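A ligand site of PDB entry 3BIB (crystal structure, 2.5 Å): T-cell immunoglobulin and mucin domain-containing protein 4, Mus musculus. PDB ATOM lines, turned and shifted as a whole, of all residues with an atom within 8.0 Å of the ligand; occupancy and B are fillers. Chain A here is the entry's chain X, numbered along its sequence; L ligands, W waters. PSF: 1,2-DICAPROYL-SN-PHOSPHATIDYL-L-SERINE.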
ATOM      1  N   SER A  29      17.639 -18.486  17.338  1.00  0.00           N
ATOM      2  CA  SER A  29      17.783 -19.890  16.990  1.00  0.00           C
ATOM      3  C   SER A  29      19.243 -20.106  16.622  1.00  0.00           C
ATOM      4  O   SER A  29      19.975 -19.137  16.405  1.00  0.00           O
ATOM      5  CB  SER A  29      16.881 -20.271  15.808  1.00  0.00           C
ATOM      6  OG  SER A  29      17.133 -19.448  14.684  1.00  0.00           O
ATOM      7  N   CYS A  31      22.500 -23.188  15.071  1.00  0.00           N
ATOM      8  CA  CYS A  31      22.912 -24.474  14.494  1.00  0.00           C
ATOM      9  C   CYS A  31      24.391 -24.694  14.720  1.00  0.00           C
ATOM     10  O   CYS A  31      25.168 -23.749  14.849  1.00  0.00           O
ATOM     11  CB  CYS A  31      22.586 -24.577  12.998  1.00  0.00           C
ATOM     12  SG  CYS A  31      23.331 -23.302  11.912  1.00  0.00           S
ATOM     13  N   PRO A  38      29.931 -20.898   6.857  1.00  0.00           N
ATOM     14  CA  PRO A  38      29.775 -20.313   5.540  1.00  0.00           C
ATOM     15  C   PRO A  38      28.956 -19.032   5.684  1.00  0.00           C
ATOM     16  O   PRO A  38      28.451 -18.748   6.772  1.00  0.00           O
ATOM     17  CB  PRO A  38      28.991 -21.382   4.788  1.00  0.00           C
ATOM     18  CG  PRO A  38      28.110 -21.985   5.859  1.00  0.00           C
ATOM     19  CD  PRO A  38      28.916 -21.942   7.129  1.00  0.00           C
ATOM     20  N   ASN A  39      28.819 -18.277   4.597  1.00  0.00           N
ATOM     21  CA  ASN A  39      28.030 -17.043   4.616  1.00  0.00           C
ATOM     22  C   ASN A  39      26.614 -17.214   5.127  1.00  0.00           C
ATOM     23  O   ASN A  39      26.083 -16.354   5.836  1.00  0.00           O
ATOM     24  CB  ASN A  39      27.996 -16.420   3.211  1.00  0.00           C
ATOM     25  CG  ASN A  39      29.336 -15.818   2.818  1.00  0.00           C
ATOM     26  OD1 ASN A  39      29.846 -16.069   1.732  1.00  0.00           O
ATOM     27  ND2 ASN A  39      29.922 -15.018   3.716  1.00  0.00           N
ATOM     28  N   SER A  40      25.997 -18.339   4.759  1.00  0.00           N
ATOM     29  CA  SER A  40      24.605 -18.601   5.085  1.00  0.00           C
ATOM     30  C   SER A  40      24.457 -19.981   5.724  1.00  0.00           C
ATOM     31  O   SER A  40      25.028 -20.968   5.250  1.00  0.00           O
ATOM     32  CB  SER A  40      23.747 -18.500   3.825  1.00  0.00           C
ATOM     33  OG  SER A  40      22.368 -18.612   4.125  1.00  0.00           O
ATOM     34  N   LYS A  41      23.695 -20.038   6.813  1.00  0.00           N
ATOM     35  CA  LYS A  41      23.366 -21.282   7.511  1.00  0.00           C
ATOM     36  C   LYS A  41      24.603 -22.029   8.019  1.00  0.00           C
ATOM     37  O   LYS A  41      25.686 -21.437   8.178  1.00  0.00           O
ATOM     38  CB  LYS A  41      22.490 -22.184   6.624  1.00  0.00           C
ATOM     39  CG  LYS A  41      21.045 -21.671   6.500  1.00  0.00           C
ATOM     40  CD  LYS A  41      20.438 -22.000   5.143  1.00  0.00           C
ATOM     41  CE  LYS A  41      19.185 -21.135   4.838  1.00  0.00           C
ATOM     42  NZ  LYS A  41      18.216 -21.061   5.972  1.00  0.00           N
ATOM     43  N   CYS A  42      24.422 -23.318   8.293  1.00  0.00           N
ATOM     44  CA  CYS A  42      25.480 -24.225   8.693  1.00  0.00           C
ATOM     45  C   CYS A  42      25.674 -25.257   7.598  1.00  0.00           C
ATOM     46  O   CYS A  42      24.695 -25.863   7.125  1.00  0.00           O
ATOM     47  CB  CYS A  42      25.093 -24.947   9.990  1.00  0.00           C
ATOM     48  SG  CYS A  42      25.224 -23.961  11.514  1.00  0.00           S
ATOM     49  N   ARG A  48      20.347 -28.389  15.231  1.00  0.00           N
ATOM     50  CA  ARG A  48      19.667 -27.118  15.105  1.00  0.00           C
ATOM     51  C   ARG A  48      18.624 -26.962  16.223  1.00  0.00           C
ATOM     52  O   ARG A  48      17.957 -27.939  16.595  1.00  0.00           O
ATOM     53  CB  ARG A  48      19.028 -27.009  13.717  1.00  0.00           C
ATOM     54  CG  ARG A  48      18.147 -25.808  13.494  1.00  0.00           C
ATOM     55  CD  ARG A  48      17.865 -25.607  12.017  1.00  0.00           C
ATOM     56  NE  ARG A  48      18.955 -24.884  11.349  1.00  0.00           N
ATOM     57  CZ  ARG A  48      19.086 -23.560  11.365  1.00  0.00           C
ATOM     58  NH1 ARG A  48      18.205 -22.805  12.012  1.00  0.00           N
ATOM     59  NH2 ARG A  48      20.100 -22.981  10.732  1.00  0.00           N
ATOM     60  N   ARG A  91      26.597 -21.210  15.059  1.00  0.00           N
ATOM     61  CA  ARG A  91      25.977 -20.044  14.454  1.00  0.00           C
ATOM     62  C   ARG A  91      24.721 -19.635  15.193  1.00  0.00           C
ATOM     63  O   ARG A  91      23.706 -20.324  15.127  1.00  0.00           O
ATOM     64  CB  ARG A  91      25.643 -20.309  12.980  1.00  0.00           C
ATOM     65  CG  ARG A  91      25.087 -19.078  12.240  1.00  0.00           C
ATOM     66  CD  ARG A  91      24.707 -19.353  10.791  1.00  0.00           C
ATOM     67  NE  ARG A  91      24.515 -18.111  10.035  1.00  0.00           N
ATOM     68  CZ  ARG A  91      25.248 -17.728   8.984  1.00  0.00           C
ATOM     69  NH1 ARG A  91      26.227 -18.490   8.499  1.00  0.00           N
ATOM     70  NH2 ARG A  91      24.986 -16.567   8.403  1.00  0.00           N
ATOM     71  N   ILE A  92      24.800 -18.499  15.908  1.00  0.00           N
ATOM     72  CA  ILE A  92      23.627 -17.895  16.521  1.00  0.00           C
ATOM     73  C   ILE A  92      22.915 -17.060  15.471  1.00  0.00           C
ATOM     74  O   ILE A  92      23.493 -16.118  14.934  1.00  0.00           O
ATOM     75  CB  ILE A  92      23.977 -17.003  17.758  1.00  0.00           C
ATOM     76  CG1 ILE A  92      24.891 -17.732  18.768  1.00  0.00           C
ATOM     77  CG2 ILE A  92      22.700 -16.458  18.431  1.00  0.00           C
ATOM     78  CD1 ILE A  92      24.326 -19.016  19.360  1.00  0.00           C
ATOM     79  N   GLU A  93      21.664 -17.404  15.185  1.00  0.00           N
ATOM     80  CA  GLU A  93      20.860 -16.668  14.204  1.00  0.00           C
ATOM     81  C   GLU A  93      20.153 -15.490  14.890  1.00  0.00           C
ATOM     82  O   GLU A  93      19.457 -15.667  15.895  1.00  0.00           O
ATOM     83  CB  GLU A  93      19.888 -17.611  13.485  1.00  0.00           C
ATOM     84  CG  GLU A  93      20.610 -18.728  12.734  1.00  0.00           C
ATOM     85  CD  GLU A  93      19.688 -19.658  11.941  1.00  0.00           C
ATOM     86  OE1 GLU A  93      18.650 -20.095  12.492  1.00  0.00           O
ATOM     87  OE2 GLU A  93      20.023 -19.975  10.774  1.00  0.00           O
ATOM     88  N   VAL A  94      20.364 -14.295  14.338  1.00  0.00           N
ATOM     89  CA  VAL A  94      19.880 -13.050  14.911  1.00  0.00           C
ATOM     90  C   VAL A  94      18.939 -12.371  13.905  1.00  0.00           C
ATOM     91  O   VAL A  94      19.259 -12.302  12.713  1.00  0.00           O
ATOM     92  CB  VAL A  94      21.082 -12.099  15.274  1.00  0.00           C
ATOM     93  CG1 VAL A  94      20.605 -10.755  15.825  1.00  0.00           C
ATOM     94  CG2 VAL A  94      22.028 -12.781  16.272  1.00  0.00           C
ATOM     95  N   PRO A  95      17.764 -11.887  14.368  1.00  0.00           N
ATOM     96  CA  PRO A  95      16.836 -11.227  13.427  1.00  0.00           C
ATOM     97  C   PRO A  95      17.454  -9.980  12.769  1.00  0.00           C
ATOM     98  O   PRO A  95      18.217  -9.251  13.408  1.00  0.00           O
ATOM     99  CB  PRO A  95      15.647 -10.845  14.304  1.00  0.00           C
ATOM    100  CG  PRO A  95      15.756 -11.712  15.517  1.00  0.00           C
ATOM    101  CD  PRO A  95      17.222 -11.903  15.737  1.00  0.00           C
ATOM    102  N   GLY A  96      17.141  -9.777  11.495  1.00  0.00           N
ATOM    103  CA  GLY A  96      17.761  -8.736  10.685  1.00  0.00           C
ATOM    104  C   GLY A  96      18.748  -9.333   9.694  1.00  0.00           C
ATOM    105  O   GLY A  96      18.921 -10.556   9.639  1.00  0.00           O
ATOM    106  N   TRP A  97      19.430  -8.469   8.930  1.00  0.00           N
ATOM    107  CA  TRP A  97      20.304  -8.925   7.852  1.00  0.00           C
ATOM    108  C   TRP A  97      21.808  -8.800   8.119  1.00  0.00           C
ATOM    109  O   TRP A  97      22.272  -7.801   8.677  1.00  0.00           O
ATOM    110  CB  TRP A  97      19.927  -8.253   6.513  1.00  0.00           C
ATOM    111  CG  TRP A  97      18.754  -8.913   5.844  1.00  0.00           C
ATOM    112  CD1 TRP A  97      17.491  -8.390   5.679  1.00  0.00           C
ATOM    113  CD2 TRP A  97      18.719 -10.220   5.248  1.00  0.00           C
ATOM    114  NE1 TRP A  97      16.686  -9.295   5.022  1.00  0.00           N
ATOM    115  CE2 TRP A  97      17.403 -10.428   4.746  1.00  0.00           C
ATOM    116  CE3 TRP A  97      19.671 -11.251   5.101  1.00  0.00           C
ATOM    117  CZ2 TRP A  97      17.019 -11.613   4.099  1.00  0.00           C
ATOM    118  CZ3 TRP A  97      19.287 -12.436   4.453  1.00  0.00           C
ATOM    119  CH2 TRP A  97      17.972 -12.599   3.958  1.00  0.00           C
ATOM    120  N   PHE A  98      22.539  -9.838   7.726  1.00  0.00           N
ATOM    121  CA  PHE A  98      23.999  -9.912   7.797  1.00  0.00           C
ATOM    122  C   PHE A  98      24.596  -9.766   9.207  1.00  0.00           C
ATOM    123  O   PHE A  98      25.714  -9.276   9.354  1.00  0.00           O
ATOM    124  CB  PHE A  98      24.670  -8.912   6.824  1.00  0.00           C
ATOM    125  CG  PHE A  98      23.978  -8.793   5.487  1.00  0.00           C
ATOM    126  CD1 PHE A  98      23.576  -9.936   4.775  1.00  0.00           C
ATOM    127  CD2 PHE A  98      23.761  -7.542   4.922  1.00  0.00           C
ATOM    128  CE1 PHE A  98      22.937  -9.826   3.535  1.00  0.00           C
ATOM    129  CE2 PHE A  98      23.136  -7.424   3.675  1.00  0.00           C
ATOM    130  CZ  PHE A  98      22.724  -8.570   2.983  1.00  0.00           C
ATOM    131  N   ASN A  99      23.873 -10.227  10.220  1.00  0.00           N
ATOM    132  CA  ASN A  99      24.297 -10.018  11.611  1.00  0.00           C
ATOM    133  C   ASN A  99      24.371 -11.264  12.519  1.00  0.00           C
ATOM    134  O   ASN A  99      24.500 -11.129  13.733  1.00  0.00           O
ATOM    135  CB  ASN A  99      23.402  -8.955  12.252  1.00  0.00           C
ATOM    136  CG  ASN A  99      21.934  -9.365  12.256  1.00  0.00           C
ATOM    137  OD1 ASN A  99      21.557 -10.344  11.618  1.00  0.00           O
ATOM    138  ND2 ASN A  99      21.106  -8.609  12.972  1.00  0.00           N
ATOM    139  N   ASP A 100      24.282 -12.464  11.947  1.00  0.00           N
ATOM    140  CA  ASP A 100      24.391 -13.706  12.727  1.00  0.00           C
ATOM    141  C   ASP A 100      25.762 -13.778  13.399  1.00  0.00           C
ATOM    142  O   ASP A 100      26.776 -13.460  12.781  1.00  0.00           O
ATOM    143  CB  ASP A 100      24.197 -14.946  11.834  1.00  0.00           C
ATOM    144  CG  ASP A 100      22.729 -15.243  11.509  1.00  0.00           C
ATOM    145  OD1 ASP A 100      21.847 -14.386  11.769  1.00  0.00           O
ATOM    146  OD2 ASP A 100      22.478 -16.339  10.970  1.00  0.00           O
ATOM    147  N   VAL A 101      25.795 -14.207  14.665  1.00  0.00           N
ATOM    148  CA  VAL A 101      27.060 -14.397  15.355  1.00  0.00           C
ATOM    149  C   VAL A 101      27.647 -15.750  14.962  1.00  0.00           C
ATOM    150  O   VAL A 101      27.141 -16.797  15.336  1.00  0.00           O
ATOM    151  CB  VAL A 101      26.953 -14.225  16.905  1.00  0.00           C
ATOM    152  CG1 VAL A 101      28.328 -14.374  17.572  1.00  0.00           C
ATOM    153  CG2 VAL A 101      26.383 -12.870  17.246  1.00  0.00           C
ATOM    154  N   LYS A 102      28.721 -15.712  14.170  1.00  0.00           N
ATOM    155  CA  LYS A 102      29.367 -16.907  13.663  1.00  0.00           C
ATOM    156  C   LYS A 102      30.644 -17.126  14.447  1.00  0.00           C
ATOM    157  O   LYS A 102      31.373 -16.183  14.708  1.00  0.00           O
ATOM    158  CB  LYS A 102      29.677 -16.765  12.176  1.00  0.00           C
ATOM    159  CG  LYS A 102      28.534 -16.198  11.338  1.00  0.00           C
ATOM    160  CD  LYS A 102      28.777 -16.342   9.848  1.00  0.00           C
ATOM    161  CE  LYS A 102      29.602 -15.206   9.287  1.00  0.00           C
ATOM    162  NZ  LYS A 102      30.047 -15.476   7.885  1.00  0.00           N
HETATM  163  O2  PSF L   1      22.908 -13.327   6.729  1.00  0.00           O
HETATM  164  O1  PSF L   1      21.949 -14.939   8.411  1.00  0.00           O
HETATM  165  P   PSF L   1      22.717 -13.533   8.315  1.00  0.00           P
HETATM  166  O4  PSF L   1      21.791 -12.456   8.819  1.00  0.00           O
HETATM  167  O3  PSF L   1      24.076 -13.683   8.948  1.00  0.00           O
HETATM  168  C2  PSF L   1      23.439 -14.402   5.957  1.00  0.00           C
HETATM  169  C3  PSF L   1      24.095 -13.899   4.675  1.00  0.00           C
HETATM  170  O11 PSF L   1      23.156 -13.260   3.823  1.00  0.00           O
HETATM  171  O12 PSF L   1      23.334 -15.044   2.308  1.00  0.00           O
HETATM  172  C1  PSF L   1      23.136 -13.841   2.480  1.00  0.00           C
HETATM  173  C4  PSF L   1      25.224 -12.946   4.980  1.00  0.00           C
HETATM  174  C5  PSF L   1      27.049 -11.976   3.613  1.00  0.00           C
HETATM  175  O51 PSF L   1      27.992 -12.699   3.895  1.00  0.00           O
HETATM  176  O52 PSF L   1      25.720 -12.524   3.720  1.00  0.00           O
HETATM  177  C6  PSF L   1      27.262 -10.543   3.154  1.00  0.00           C
HETATM  178  C13 PSF L   1      22.869 -12.963   1.277  1.00  0.00           C
HETATM  179  C14 PSF L   1      24.178 -12.519   0.629  1.00  0.00           C
HETATM  180  C15 PSF L   1      24.079 -12.567  -0.897  1.00  0.00           C
HETATM  181  N   PSF L   1      20.155 -16.927   9.479  1.00  0.00           N
HETATM  182  CA  PSF L   1      20.197 -16.581   8.082  1.00  0.00           C
HETATM  183  CB  PSF L   1      20.605 -15.110   7.950  1.00  0.00           C
HETATM  184  C   PSF L   1      21.202 -17.450   7.370  1.00  0.00           C
HETATM  185  OT1 PSF L   1      21.814 -18.320   8.027  1.00  0.00           O
HETATM  186  OT2 PSF L   1      21.405 -17.279   6.153  1.00  0.00           O
HETATM  187  C16 PSF L   1      23.924 -11.180  -1.490  1.00  0.00           C
HETATM  188  C17 PSF L   1      25.162 -10.748  -2.237  1.00  0.00           C
HETATM  189  O   HOH W   1      18.848 -14.551  10.773  1.00  0.00           O
HETATM  190  O   HOH W   2      26.243 -12.557   8.360  1.00  0.00           O
HETATM  191  O   HOH W   3      27.722 -14.320   6.695  1.00  0.00           O
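Water W2 lies within hydrogen-bond range of an oxygen (O3) of the ligand (2.5 Å) and the backbone carbonyl oxygen of Phe 98 (3.5 Å).
Water W1 lies within hydrogen-bond range of the backbone carbonyl oxygen of Val 94 (3.0 Å), a nitrogen (N) of the ligand (3.0 Å) and the side-chain carboxylate of Asp 100 (3.2 Å).
Water W3 lies within hydrogen-bond range of the backbone carbonyl oxygen of Asn 39, the side-chain amino group of Lys 102 and an oxygen (O51) of the ligand.
The backbone NH (N) of Asn 99 sits at hydrogen-bond distance from an oxygen (O4) of the ligand, at 3.4 Å.
An oxygen (OT2) of the ligand lies within hydrogen-bond range of the side-chain hydroxyl (OG) of Ser 40.
The side-chain carboxylate (OE2) of Glu 93 is in salt-bridge range of a nitrogen (N) of the ligand (3.3 Å).
ND2 of Asn 39 is in hydrogen-bond range of O51 of the ligand.
A nitrogen (N) of the ligand is in salt-bridge range of the side-chain carboxylate of Asp 100, at 2.8 Å.
N of Phe 98 is in hydrogen-bond range of O4 of the ligand, at 2.9 Å.
N of Asp 100 lies close to O3 of the ligand.
The guanidinium group (NH2) of Arg 91 is in salt-bridge range of an oxygen (O3) of the ligand (3.1 Å).
The backbone NH of Lys 41 lies within hydrogen-bond range of an oxygen (OT1) of the ligand, at 2.8 Å.
Merely in contact with the ligand: Gly 96 (3.5 Å) and Trp 97 (3.7 Å).
Within 4 Å of the ligand: Asn 39, Ser 40, Lys 41, Arg 91, Glu 93, Gly 96, Trp 97, Phe 98, Asn 99 and Asp 100.
The side-chain amide nitrogen (ND2) of Asn 99 is in hydrogen-bond range of the backbone carbonyl oxygen (O) of Pro 95.
The backbone NH (N) of Arg 91 is in hydrogen-bond range of the backbone carbonyl oxygen (O) of Cys 31.
OD1 of Asn 99 sits close to O of Gly 96, 3.3 Å away.
The backbone carbonyl oxygen (O) of Asn 39 is in hydrogen-bond range of the guanidinium group (NH2) of Arg 91 (2.8 Å).
The side-chain sulfur (SG) of Cys 31 forms a disulfide with the side-chain sulfur (SG) of Cys 42 (2.0 Å).
The backbone carbonyl oxygen of Lys 41 lies within hydrogen-bond range of the guanidinium group of Arg 91, at 3.0 Å.
N of Glu 93 sits at hydrogen-bond distance from O of Ser 29 (2.7 Å).
NH1 of Arg 91 is in hydrogen-bond range of O of Pro 38 (2.8 Å).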
